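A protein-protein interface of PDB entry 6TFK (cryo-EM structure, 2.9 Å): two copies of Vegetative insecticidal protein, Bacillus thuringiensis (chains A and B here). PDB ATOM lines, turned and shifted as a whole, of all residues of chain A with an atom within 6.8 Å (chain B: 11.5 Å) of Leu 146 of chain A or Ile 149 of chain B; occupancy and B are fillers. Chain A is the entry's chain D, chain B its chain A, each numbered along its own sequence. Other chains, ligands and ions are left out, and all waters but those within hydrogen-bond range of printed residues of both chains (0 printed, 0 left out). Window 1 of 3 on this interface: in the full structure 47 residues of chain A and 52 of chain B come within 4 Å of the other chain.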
ATOM      1  N   TYR A 141      26.649 -34.343   7.777  1.00  0.00           N
ATOM      2  CA  TYR A 141      25.602 -35.141   7.145  1.00  0.00           C
ATOM      3  C   TYR A 141      24.234 -34.490   7.325  1.00  0.00           C
ATOM      4  O   TYR A 141      23.416 -34.471   6.396  1.00  0.00           O
ATOM      5  CB  TYR A 141      25.607 -36.557   7.717  1.00  0.00           C
ATOM      6  CG  TYR A 141      24.569 -37.465   7.103  1.00  0.00           C
ATOM      7  CD1 TYR A 141      24.578 -37.741   5.743  1.00  0.00           C
ATOM      8  CD2 TYR A 141      23.586 -38.054   7.884  1.00  0.00           C
ATOM      9  CE1 TYR A 141      23.631 -38.571   5.178  1.00  0.00           C
ATOM     10  CE2 TYR A 141      22.637 -38.887   7.328  1.00  0.00           C
ATOM     11  CZ  TYR A 141      22.664 -39.142   5.974  1.00  0.00           C
ATOM     12  OH  TYR A 141      21.720 -39.971   5.416  1.00  0.00           O
ATOM     13  N   LEU A 142      23.966 -33.957   8.519  1.00  0.00           N
ATOM     14  CA  LEU A 142      22.713 -33.241   8.741  1.00  0.00           C
ATOM     15  C   LEU A 142      22.588 -32.046   7.805  1.00  0.00           C
ATOM     16  O   LEU A 142      21.504 -31.770   7.277  1.00  0.00           O
ATOM     17  CB  LEU A 142      22.611 -32.775  10.193  1.00  0.00           C
ATOM     18  CG  LEU A 142      22.409 -33.820  11.291  1.00  0.00           C
ATOM     19  CD1 LEU A 142      22.153 -33.119  12.614  1.00  0.00           C
ATOM     20  CD2 LEU A 142      21.273 -34.771  10.966  1.00  0.00           C
ATOM     21  N   SER A 143      23.683 -31.312   7.602  1.00  0.00           N
ATOM     22  CA  SER A 143      23.633 -30.155   6.714  1.00  0.00           C
ATOM     23  C   SER A 143      23.352 -30.581   5.279  1.00  0.00           C
ATOM     24  O   SER A 143      22.614 -29.903   4.554  1.00  0.00           O
ATOM     25  CB  SER A 143      24.941 -29.372   6.794  1.00  0.00           C
ATOM     26  OG  SER A 143      26.006 -30.102   6.214  1.00  0.00           O
ATOM     27  N   LYS A 144      23.933 -31.703   4.850  1.00  0.00           N
ATOM     28  CA  LYS A 144      23.625 -32.218   3.518  1.00  0.00           C
ATOM     29  C   LYS A 144      22.150 -32.587   3.403  1.00  0.00           C
ATOM     30  O   LYS A 144      21.500 -32.294   2.388  1.00  0.00           O
ATOM     31  CB  LYS A 144      24.506 -33.425   3.205  1.00  0.00           C
ATOM     32  CG  LYS A 144      25.977 -33.084   3.040  1.00  0.00           C
ATOM     33  CD  LYS A 144      26.820 -34.331   2.840  1.00  0.00           C
ATOM     34  CE  LYS A 144      28.299 -33.992   2.738  1.00  0.00           C
ATOM     35  NZ  LYS A 144      29.154 -35.211   2.718  1.00  0.00           N
ATOM     36  N   GLN A 145      21.607 -33.242   4.431  1.00  0.00           N
ATOM     37  CA  GLN A 145      20.182 -33.561   4.435  1.00  0.00           C
ATOM     38  C   GLN A 145      19.340 -32.299   4.309  1.00  0.00           C
ATOM     39  O   GLN A 145      18.363 -32.259   3.552  1.00  0.00           O
ATOM     40  CB  GLN A 145      19.815 -34.318   5.711  1.00  0.00           C
ATOM     41  CG  GLN A 145      20.277 -35.760   5.742  1.00  0.00           C
ATOM     42  CD  GLN A 145      19.666 -36.533   6.893  1.00  0.00           C
ATOM     43  OE1 GLN A 145      19.129 -35.946   7.830  1.00  0.00           O
ATOM     44  NE2 GLN A 145      19.736 -37.855   6.822  1.00  0.00           N
ATOM     45  N   LEU A 146      19.701 -31.255   5.055  1.00  0.00           N
ATOM     46  CA  LEU A 146      18.939 -30.012   4.999  1.00  0.00           C
ATOM     47  C   LEU A 146      19.046 -29.345   3.634  1.00  0.00           C
ATOM     48  O   LEU A 146      18.076 -28.739   3.166  1.00  0.00           O
ATOM     49  CB  LEU A 146      19.412 -29.054   6.090  1.00  0.00           C
ATOM     50  CG  LEU A 146      18.973 -29.402   7.512  1.00  0.00           C
ATOM     51  CD1 LEU A 146      19.636 -28.473   8.505  1.00  0.00           C
ATOM     52  CD2 LEU A 146      17.465 -29.324   7.643  1.00  0.00           C
ATOM     53  N   GLN A 147      20.203 -29.439   2.981  1.00  0.00           N
ATOM     54  CA  GLN A 147      20.316 -28.890   1.634  1.00  0.00           C
ATOM     55  C   GLN A 147      19.422 -29.644   0.658  1.00  0.00           C
ATOM     56  O   GLN A 147      18.756 -29.032  -0.188  1.00  0.00           O
ATOM     57  CB  GLN A 147      21.771 -28.924   1.168  1.00  0.00           C
ATOM     58  CG  GLN A 147      22.451 -27.568   1.199  1.00  0.00           C
ATOM     59  CD  GLN A 147      21.791 -26.569   0.269  1.00  0.00           C
ATOM     60  OE1 GLN A 147      21.334 -26.925  -0.817  1.00  0.00           O
ATOM     61  NE2 GLN A 147      21.726 -25.314   0.696  1.00  0.00           N
ATOM     62  N   GLU A 148      19.397 -30.975   0.757  1.00  0.00           N
ATOM     63  CA  GLU A 148      18.480 -31.745  -0.078  1.00  0.00           C
ATOM     64  C   GLU A 148      17.032 -31.347   0.192  1.00  0.00           C
ATOM     65  O   GLU A 148      16.218 -31.255  -0.735  1.00  0.00           O
ATOM     66  CB  GLU A 148      18.681 -33.240   0.160  1.00  0.00           C
ATOM     67  CG  GLU A 148      20.054 -33.744  -0.251  1.00  0.00           C
ATOM     68  CD  GLU A 148      20.200 -35.243  -0.086  1.00  0.00           C
ATOM     69  OE1 GLU A 148      19.214 -35.898   0.314  1.00  0.00           O
ATOM     70  OE2 GLU A 148      21.300 -35.768  -0.358  1.00  0.00           O
ATOM     71  N   ILE A 149      16.698 -31.099   1.459  1.00  0.00           N
ATOM     72  CA  ILE A 149      15.339 -30.692   1.802  1.00  0.00           C
ATOM     73  C   ILE A 149      15.012 -29.337   1.185  1.00  0.00           C
ATOM     74  O   ILE A 149      13.900 -29.116   0.694  1.00  0.00           O
ATOM     75  CB  ILE A 149      15.161 -30.680   3.329  1.00  0.00           C
ATOM     76  CG1 ILE A 149      14.988 -32.110   3.845  1.00  0.00           C
ATOM     77  CG2 ILE A 149      13.977 -29.809   3.720  1.00  0.00           C
ATOM     78  CD1 ILE A 149      15.048 -32.234   5.347  1.00  0.00           C
ATOM     79  N   SER A 150      15.967 -28.407   1.206  1.00  0.00           N
ATOM     80  CA  SER A 150      15.727 -27.098   0.605  1.00  0.00           C
ATOM     81  C   SER A 150      15.533 -27.214  -0.901  1.00  0.00           C
ATOM     82  O   SER A 150      14.696 -26.515  -1.487  1.00  0.00           O
ATOM     83  CB  SER A 150      16.883 -26.153   0.927  1.00  0.00           C
ATOM     84  OG  SER A 150      18.078 -26.586   0.304  1.00  0.00           O
ATOM     85  N   ASP A 151      16.297 -28.096  -1.550  1.00  0.00           N
ATOM     86  CA  ASP A 151      16.090 -28.331  -2.976  1.00  0.00           C
ATOM     87  C   ASP A 151      14.697 -28.890  -3.244  1.00  0.00           C
ATOM     88  O   ASP A 151      14.009 -28.460  -4.183  1.00  0.00           O
ATOM     89  CB  ASP A 151      17.160 -29.281  -3.513  1.00  0.00           C
ATOM     90  CG  ASP A 151      18.552 -28.685  -3.453  1.00  0.00           C
ATOM     91  OD1 ASP A 151      18.676 -27.496  -3.090  1.00  0.00           O
ATOM     92  OD2 ASP A 151      19.522 -29.404  -3.767  1.00  0.00           O
ATOM     93  N   LEU A 153      12.101 -28.383  -1.459  1.00  0.00           N
ATOM     94  CA  LEU A 153      11.149 -27.299  -1.241  1.00  0.00           C
ATOM     95  C   LEU A 153      11.094 -26.366  -2.443  1.00  0.00           C
ATOM     96  O   LEU A 153      10.015 -25.892  -2.818  1.00  0.00           O
ATOM     97  CB  LEU A 153      11.518 -26.520   0.019  1.00  0.00           C
ATOM     98  CG  LEU A 153      11.315 -27.260   1.340  1.00  0.00           C
ATOM     99  CD1 LEU A 153      11.882 -26.453   2.485  1.00  0.00           C
ATOM    100  CD2 LEU A 153       9.844 -27.551   1.574  1.00  0.00           C
ATOM    101  N   LEU B 137      29.328 -23.443  16.228  1.00  0.00           N
ATOM    102  CA  LEU B 137      29.142 -22.679  14.996  1.00  0.00           C
ATOM    103  C   LEU B 137      28.394 -23.499  13.950  1.00  0.00           C
ATOM    104  O   LEU B 137      27.504 -22.983  13.258  1.00  0.00           O
ATOM    105  CB  LEU B 137      30.494 -22.222  14.448  1.00  0.00           C
ATOM    106  CG  LEU B 137      31.311 -21.283  15.339  1.00  0.00           C
ATOM    107  CD1 LEU B 137      32.581 -20.857  14.622  1.00  0.00           C
ATOM    108  CD2 LEU B 137      30.496 -20.068  15.758  1.00  0.00           C
ATOM    109  N   GLN B 138      28.750 -24.778  13.810  1.00  0.00           N
ATOM    110  CA  GLN B 138      28.037 -25.640  12.873  1.00  0.00           C
ATOM    111  C   GLN B 138      26.553 -25.714  13.212  1.00  0.00           C
ATOM    112  O   GLN B 138      25.699 -25.680  12.317  1.00  0.00           O
ATOM    113  CB  GLN B 138      28.648 -27.040  12.870  1.00  0.00           C
ATOM    114  CG  GLN B 138      29.968 -27.143  12.131  1.00  0.00           C
ATOM    115  CD  GLN B 138      30.362 -28.579  11.851  1.00  0.00           C
ATOM    116  OE1 GLN B 138      29.719 -29.514  12.322  1.00  0.00           O
ATOM    117  NE2 GLN B 138      31.423 -28.759  11.076  1.00  0.00           N
ATOM    118  N   ILE B 139      26.226 -25.817  14.500  1.00  0.00           N
ATOM    119  CA  ILE B 139      24.823 -25.921  14.886  1.00  0.00           C
ATOM    120  C   ILE B 139      24.097 -24.604  14.650  1.00  0.00           C
ATOM    121  O   ILE B 139      22.911 -24.596  14.298  1.00  0.00           O
ATOM    122  CB  ILE B 139      24.703 -26.381  16.349  1.00  0.00           C
ATOM    123  CG1 ILE B 139      25.124 -27.847  16.465  1.00  0.00           C
ATOM    124  CG2 ILE B 139      23.280 -26.170  16.851  1.00  0.00           C
ATOM    125  CD1 ILE B 139      25.124 -28.381  17.878  1.00  0.00           C
ATOM    126  N   GLU B 140      24.778 -23.471  14.830  1.00  0.00           N
ATOM    127  CA  GLU B 140      24.159 -22.195  14.482  1.00  0.00           C
ATOM    128  C   GLU B 140      23.864 -22.125  12.988  1.00  0.00           C
ATOM    129  O   GLU B 140      22.810 -21.623  12.573  1.00  0.00           O
ATOM    130  CB  GLU B 140      25.057 -21.035  14.907  1.00  0.00           C
ATOM    131  CG  GLU B 140      25.089 -20.801  16.407  1.00  0.00           C
ATOM    132  CD  GLU B 140      25.728 -19.479  16.777  1.00  0.00           C
ATOM    133  OE1 GLU B 140      26.194 -18.765  15.864  1.00  0.00           O
ATOM    134  OE2 GLU B 140      25.763 -19.151  17.981  1.00  0.00           O
ATOM    135  N   TYR B 141      24.787 -22.624  12.163  1.00  0.00           N
ATOM    136  CA  TYR B 141      24.527 -22.679  10.728  1.00  0.00           C
ATOM    137  C   TYR B 141      23.327 -23.570  10.422  1.00  0.00           C
ATOM    138  O   TYR B 141      22.497 -23.240   9.564  1.00  0.00           O
ATOM    139  CB  TYR B 141      25.771 -23.175   9.992  1.00  0.00           C
ATOM    140  CG  TYR B 141      25.606 -23.242   8.493  1.00  0.00           C
ATOM    141  CD1 TYR B 141      25.317 -22.103   7.756  1.00  0.00           C
ATOM    142  CD2 TYR B 141      25.750 -24.442   7.814  1.00  0.00           C
ATOM    143  CE1 TYR B 141      25.168 -22.159   6.385  1.00  0.00           C
ATOM    144  CE2 TYR B 141      25.603 -24.508   6.443  1.00  0.00           C
ATOM    145  CZ  TYR B 141      25.312 -23.364   5.733  1.00  0.00           C
ATOM    146  OH  TYR B 141      25.164 -23.426   4.368  1.00  0.00           O
ATOM    147  N   LEU B 142      23.223 -24.708  11.112  1.00  0.00           N
ATOM    148  CA  LEU B 142      22.057 -25.570  10.940  1.00  0.00           C
ATOM    149  C   LEU B 142      20.772 -24.834  11.300  1.00  0.00           C
ATOM    150  O   LEU B 142      19.751 -24.978  10.617  1.00  0.00           O
ATOM    151  CB  LEU B 142      22.191 -26.829  11.795  1.00  0.00           C
ATOM    152  CG  LEU B 142      23.231 -27.880  11.404  1.00  0.00           C
ATOM    153  CD1 LEU B 142      23.065 -29.105  12.285  1.00  0.00           C
ATOM    154  CD2 LEU B 142      23.127 -28.260   9.940  1.00  0.00           C
ATOM    155  N   SER B 143      20.795 -24.060  12.385  1.00  0.00           N
ATOM    156  CA  SER B 143      19.599 -23.328  12.788  1.00  0.00           C
ATOM    157  C   SER B 143      19.220 -22.287  11.743  1.00  0.00           C
ATOM    158  O   SER B 143      18.034 -22.072  11.467  1.00  0.00           O
ATOM    159  CB  SER B 143      19.816 -22.668  14.147  1.00  0.00           C
ATOM    160  OG  SER B 143      20.752 -21.611  14.055  1.00  0.00           O
ATOM    161  N   LYS B 144      20.215 -21.626  11.150  1.00  0.00           N
ATOM    162  CA  LYS B 144      19.923 -20.686  10.070  1.00  0.00           C
ATOM    163  C   LYS B 144      19.296 -21.399   8.878  1.00  0.00           C
ATOM    164  O   LYS B 144      18.332 -20.901   8.276  1.00  0.00           O
ATOM    165  CB  LYS B 144      21.198 -19.957   9.649  1.00  0.00           C
ATOM    166  CG  LYS B 144      21.739 -19.010  10.707  1.00  0.00           C
ATOM    167  CD  LYS B 144      23.062 -18.397  10.282  1.00  0.00           C
ATOM    168  CE  LYS B 144      23.633 -17.500  11.369  1.00  0.00           C
ATOM    169  NZ  LYS B 144      25.009 -17.033  11.044  1.00  0.00           N
ATOM    170  N   GLN B 145      19.836 -22.565   8.515  1.00  0.00           N
ATOM    171  CA  GLN B 145      19.244 -23.351   7.436  1.00  0.00           C
ATOM    172  C   GLN B 145      17.791 -23.689   7.743  1.00  0.00           C
ATOM    173  O   GLN B 145      16.917 -23.590   6.874  1.00  0.00           O
ATOM    174  CB  GLN B 145      20.050 -24.630   7.212  1.00  0.00           C
ATOM    175  CG  GLN B 145      21.377 -24.422   6.513  1.00  0.00           C
ATOM    176  CD  GLN B 145      22.006 -25.731   6.079  1.00  0.00           C
ATOM    177  OE1 GLN B 145      21.606 -26.802   6.532  1.00  0.00           O
ATOM    178  NE2 GLN B 145      22.988 -25.651   5.193  1.00  0.00           N
ATOM    179  N   LEU B 146      17.515 -24.102   8.981  1.00  0.00           N
ATOM    180  CA  LEU B 146      16.150 -24.456   9.352  1.00  0.00           C
ATOM    181  C   LEU B 146      15.223 -23.248   9.319  1.00  0.00           C
ATOM    182  O   LEU B 146      14.050 -23.380   8.957  1.00  0.00           O
ATOM    183  CB  LEU B 146      16.130 -25.096  10.737  1.00  0.00           C
ATOM    184  CG  LEU B 146      16.660 -26.527  10.813  1.00  0.00           C
ATOM    185  CD1 LEU B 146      16.748 -26.977  12.256  1.00  0.00           C
ATOM    186  CD2 LEU B 146      15.775 -27.472  10.023  1.00  0.00           C
ATOM    187  N   GLN B 147      15.721 -22.069   9.690  1.00  0.00           N
ATOM    188  CA  GLN B 147      14.891 -20.872   9.590  1.00  0.00           C
ATOM    189  C   GLN B 147      14.566 -20.555   8.136  1.00  0.00           C
ATOM    190  O   GLN B 147      13.423 -20.203   7.809  1.00  0.00           O
ATOM    191  CB  GLN B 147      15.586 -19.687  10.258  1.00  0.00           C
ATOM    192  CG  GLN B 147      15.002 -19.326  11.611  1.00  0.00           C
ATOM    193  CD  GLN B 147      13.552 -18.897  11.519  1.00  0.00           C
ATOM    194  OE1 GLN B 147      13.143 -18.256  10.551  1.00  0.00           O
ATOM    195  NE2 GLN B 147      12.762 -19.260  12.522  1.00  0.00           N
ATOM    196  N   GLU B 148      15.555 -20.668   7.249  1.00  0.00           N
ATOM    197  CA  GLU B 148      15.278 -20.481   5.827  1.00  0.00           C
ATOM    198  C   GLU B 148      14.250 -21.493   5.334  1.00  0.00           C
ATOM    199  O   GLU B 148      13.369 -21.161   4.530  1.00  0.00           O
ATOM    200  CB  GLU B 148      16.571 -20.588   5.021  1.00  0.00           C
ATOM    201  CG  GLU B 148      17.582 -19.501   5.340  1.00  0.00           C
ATOM    202  CD  GLU B 148      18.820 -19.582   4.469  1.00  0.00           C
ATOM    203  OE1 GLU B 148      18.870 -20.462   3.583  1.00  0.00           O
ATOM    204  OE2 GLU B 148      19.743 -18.764   4.669  1.00  0.00           O
ATOM    205  N   ILE B 149      14.341 -22.734   5.814  1.00  0.00           N
ATOM    206  CA  ILE B 149      13.384 -23.758   5.410  1.00  0.00           C
ATOM    207  C   ILE B 149      11.983 -23.404   5.892  1.00  0.00           C
ATOM    208  O   ILE B 149      10.997 -23.599   5.172  1.00  0.00           O
ATOM    209  CB  ILE B 149      13.832 -25.135   5.928  1.00  0.00           C
ATOM    210  CG1 ILE B 149      14.970 -25.673   5.058  1.00  0.00           C
ATOM    211  CG2 ILE B 149      12.658 -26.101   5.959  1.00  0.00           C
ATOM    212  CD1 ILE B 149      15.641 -26.904   5.615  1.00  0.00           C
ATOM    213  N   SER B 150      11.866 -22.888   7.116  1.00  0.00           N
ATOM    214  CA  SER B 150      10.554 -22.504   7.625  1.00  0.00           C
ATOM    215  C   SER B 150       9.973 -21.346   6.820  1.00  0.00           C
ATOM    216  O   SER B 150       8.763 -21.301   6.563  1.00  0.00           O
ATOM    217  CB  SER B 150      10.652 -22.135   9.103  1.00  0.00           C
ATOM    218  OG  SER B 150      11.425 -20.964   9.284  1.00  0.00           O
ATOM    219  N   ASP B 151      10.821 -20.400   6.411  1.00  0.00           N
ATOM    220  CA  ASP B 151      10.346 -19.322   5.547  1.00  0.00           C
ATOM    221  C   ASP B 151       9.846 -19.867   4.214  1.00  0.00           C
ATOM    222  O   ASP B 151       8.789 -19.451   3.714  1.00  0.00           O
ATOM    223  CB  ASP B 151      11.462 -18.302   5.324  1.00  0.00           C
ATOM    224  CG  ASP B 151      11.857 -17.580   6.597  1.00  0.00           C
ATOM    225  OD1 ASP B 151      11.196 -17.799   7.634  1.00  0.00           O
ATOM    226  OD2 ASP B 151      12.828 -16.797   6.562  1.00  0.00           O
ATOM    227  N   LYS B 152      10.600 -20.793   3.617  1.00  0.00           N
ATOM    228  CA  LYS B 152      10.148 -21.419   2.379  1.00  0.00           C
ATOM    229  C   LYS B 152       8.811 -22.120   2.577  1.00  0.00           C
ATOM    230  O   LYS B 152       7.946 -22.081   1.696  1.00  0.00           O
ATOM    231  CB  LYS B 152      11.194 -22.410   1.874  1.00  0.00           C
ATOM    232  CG  LYS B 152      12.460 -21.766   1.358  1.00  0.00           C
ATOM    233  CD  LYS B 152      13.343 -22.782   0.661  1.00  0.00           C
ATOM    234  CE  LYS B 152      14.619 -22.145   0.151  1.00  0.00           C
ATOM    235  NZ  LYS B 152      15.385 -23.072  -0.719  1.00  0.00           N
ATOM    236  N   LEU B 153       8.626 -22.773   3.724  1.00  0.00           N
ATOM    237  CA  LEU B 153       7.366 -23.460   3.984  1.00  0.00           C
ATOM    238  C   LEU B 153       6.214 -22.471   4.102  1.00  0.00           C
ATOM    239  O   LEU B 153       5.105 -22.741   3.627  1.00  0.00           O
ATOM    240  CB  LEU B 153       7.477 -24.302   5.252  1.00  0.00           C
ATOM    241  CG  LEU B 153       8.385 -25.527   5.159  1.00  0.00           C
ATOM    242  CD1 LEU B 153       8.543 -26.166   6.518  1.00  0.00           C
ATOM    243  CD2 LEU B 153       7.835 -26.530   4.161  1.00  0.00           C
ATOM    244  N   ASP B 154       6.452 -21.328   4.745  1.00  0.00           N
ATOM    245  CA  ASP B 154       5.422 -20.295   4.805  1.00  0.00           C
ATOM    246  C   ASP B 154       5.032 -19.836   3.405  1.00  0.00           C
ATOM    247  O   ASP B 154       3.842 -19.710   3.081  1.00  0.00           O
ATOM    248  CB  ASP B 154       5.913 -19.114   5.640  1.00  0.00           C
ATOM    249  CG  ASP B 154       6.194 -19.494   7.077  1.00  0.00           C
ATOM    250  OD1 ASP B 154       6.043 -20.686   7.418  1.00  0.00           O
ATOM    251  OD2 ASP B 154       6.562 -18.602   7.870  1.00  0.00           O
ATOM    252  N   ILE B 155       6.030 -19.579   2.557  1.00  0.00           N
ATOM    253  CA  ILE B 155       5.743 -19.145   1.191  1.00  0.00           C
ATOM    254  C   ILE B 155       4.953 -20.214   0.445  1.00  0.00           C
ATOM    255  O   ILE B 155       4.004 -19.910  -0.289  1.00  0.00           O
ATOM    256  CB  ILE B 155       7.049 -18.793   0.456  1.00  0.00           C
ATOM    257  CG1 ILE B 155       7.725 -17.596   1.126  1.00  0.00           C
ATOM    258  CG2 ILE B 155       6.766 -18.502  -1.012  1.00  0.00           C
ATOM    259  CD1 ILE B 155       9.108 -17.293   0.593  1.00  0.00           C
ATOM    260  N   ILE B 156       5.328 -21.482   0.622  1.00  0.00           N
ATOM    261  CA  ILE B 156       4.647 -22.564  -0.081  1.00  0.00           C
ATOM    262  C   ILE B 156       3.201 -22.677   0.381  1.00  0.00           C
ATOM    263  O   ILE B 156       2.294 -22.914  -0.426  1.00  0.00           O
ATOM    264  CB  ILE B 156       5.408 -23.887   0.115  1.00  0.00           C
ATOM    265  CG1 ILE B 156       6.758 -23.830  -0.599  1.00  0.00           C
ATOM    266  CG2 ILE B 156       4.581 -25.053  -0.400  1.00  0.00           C
ATOM    267  CD1 ILE B 156       7.709 -24.931  -0.201  1.00  0.00           C
ATOM    268  N   ASN B 157       2.957 -22.522   1.683  1.00  0.00           N
ATOM    269  CA  ASN B 157       1.587 -22.598   2.179  1.00  0.00           C
ATOM    270  C   ASN B 157       0.746 -21.454   1.630  1.00  0.00           C
ATOM    271  O   ASN B 157      -0.417 -21.652   1.250  1.00  0.00           O
ATOM    272  CB  ASN B 157       1.579 -22.585   3.706  1.00  0.00           C
ATOM    273  CG  ASN B 157       0.234 -22.974   4.281  1.00  0.00           C
ATOM    274  OD1 ASN B 157      -0.507 -23.752   3.684  1.00  0.00           O
ATOM    275  ND2 ASN B 157      -0.090 -22.432   5.447  1.00  0.00           N
ATOM    276  N   VAL B 158       1.315 -20.249   1.581  1.00  0.00           N
ATOM    277  CA  VAL B 158       0.582 -19.128   1.001  1.00  0.00           C
ATOM    278  C   VAL B 158       0.263 -19.404  -0.463  1.00  0.00           C
ATOM    279  O   VAL B 158      -0.837 -19.103  -0.941  1.00  0.00           O
ATOM    280  CB  VAL B 158       1.376 -17.821   1.176  1.00  0.00           C
ATOM    281  CG1 VAL B 158       0.797 -16.723   0.302  1.00  0.00           C
ATOM    282  CG2 VAL B 158       1.366 -17.402   2.634  1.00  0.00           C
ATOM    283  N   LYS B 258       3.296 -11.280   2.419  1.00  0.00           N
ATOM    284  CA  LYS B 258       4.529 -12.018   2.156  1.00  0.00           C
ATOM    285  C   LYS B 258       5.383 -11.317   1.104  1.00  0.00           C
ATOM    286  O   LYS B 258       6.538 -10.963   1.364  1.00  0.00           O
ATOM    287  CB  LYS B 258       4.208 -13.447   1.713  1.00  0.00           C
ATOM    288  CG  LYS B 258       3.557 -14.305   2.783  1.00  0.00           C
ATOM    289  CD  LYS B 258       4.468 -14.526   3.981  1.00  0.00           C
ATOM    290  CE  LYS B 258       3.784 -15.370   5.044  1.00  0.00           C
ATOM    291  NZ  LYS B 258       2.557 -14.714   5.574  1.00  0.00           N
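Ser 143 of chain A touches Leu 142 of chain B, but with the chains exchanged Leu 142 of chain A does not touch Ser 143 of chain B (9.2 Å).
Leu 146 of chain A touches its own counterpart, Leu 146 of chain B.
Ile 149 of chain A touches its own counterpart, Ile 149 of chain B.
Leu 153 of chain A touches Ile 149 of chain B, but with the chains exchanged Ile 149 of chain A does not touch Leu 153 of chain B (7.0 Å).
Of the 11 pairs that touch across the chains among the printed residues, 3 have their exchanged pair printed and touching as well.
Leu 142 of chain B touches Ser 143 of chain A (CD2 to CA, 3.8 Å).
OE1 of Gln 145 of chain B touches O of Ser 143 of chain A, at 3.8 Å.
Leu 146 of chain A touches Leu 142 of chain B.
CB of Leu 146 of chain A touches OE1 of Gln 145 of chain B, 3.2 Å away.
Leu 146 of chain A touches Leu 146 of chain B.
Leu 146 of chain A touches Ile 149 of chain B.
Ile 149 of chain A touches Ile 149 of chain B.
Ser 150 of chain A touches Lys 152 of chain B.
CD2 of Leu 153 of chain A touches CD2 of Leu 153 of chain B, at 3.4 Å.
Leu 153 of chain A touches Ile 156 of chain B (O to CD1, 3.6 Å).
The side-chain hydroxyl (OH) of Tyr 141 of chain B lies close to the side-chain amide nitrogen (NE2) of Gln 145 of chain B.
The backbone carbonyl oxygen (O) of Gln 147 of chain A lies within hydrogen-bond range of the side-chain hydroxyl (OG) of Ser 150 of chain A.
No residue of chain B comes within 4 Å of Leu 142 of chain A.
Ser 143 of chain A touches just these residues of chain B: Leu 142 and Gln 145.
Leu 146 of chain A touches just these residues of chain B: Leu 142 (3.8 Å), Gln 145 (3.2 Å), Leu 146 (3.5 Å) and Ile 149 (3.6 Å).
Gln 147 of chain A touches none of the printed residues of chain B.
No residue of chain B comes within 4 Å of Glu 148 of chain A.
Ile 149 of chain A touches just one residue of chain B: Ile 149.
Printed residues of chain B within 4 Å of Leu 153 of chain A: Ile 149, Leu 153 and Ile 156.
Printed residues of chain A within 4 Å of Leu 142 of chain B: Ser 143 and Leu 146.
Of chain A, only Leu 146 (3.6 Å), Ile 149 (3.8 Å) and Leu 153 (3.6 Å) come within 4 Å of Ile 149 of chain B.
Asp 151 of chain B touches none of the printed residues of chain A.
Of the printed residues of chain A, Lys 152 of chain B touches Ser 150.
Printed residues of chain A within 4 Å of Leu 153 of chain B: Leu 153.
Printed residues of chain A within 4 Å of Ile 156 of chain B: Leu 153 (3.6 Å).
The nearest residue of chain B that does not touch Leu 146 of chain A is Ser 143 of chain B (6.0 Å).
The nearest printed residue of chain B that does not touch Leu 153 of chain A is Lys 152 of chain B (4.1 Å).
Of the 12 printed residues of chain A, 5 touch a printed residue of chain B.
Printed residues of chain A that touch a printed residue of chain B: Ser 143, Leu 146, Ile 149, Ser 150 and Leu 153.
Among the printed residues, no Asp or Glu carboxylate lies within 4 Å of a Lys or Arg side-chain nitrogen of the other chain.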
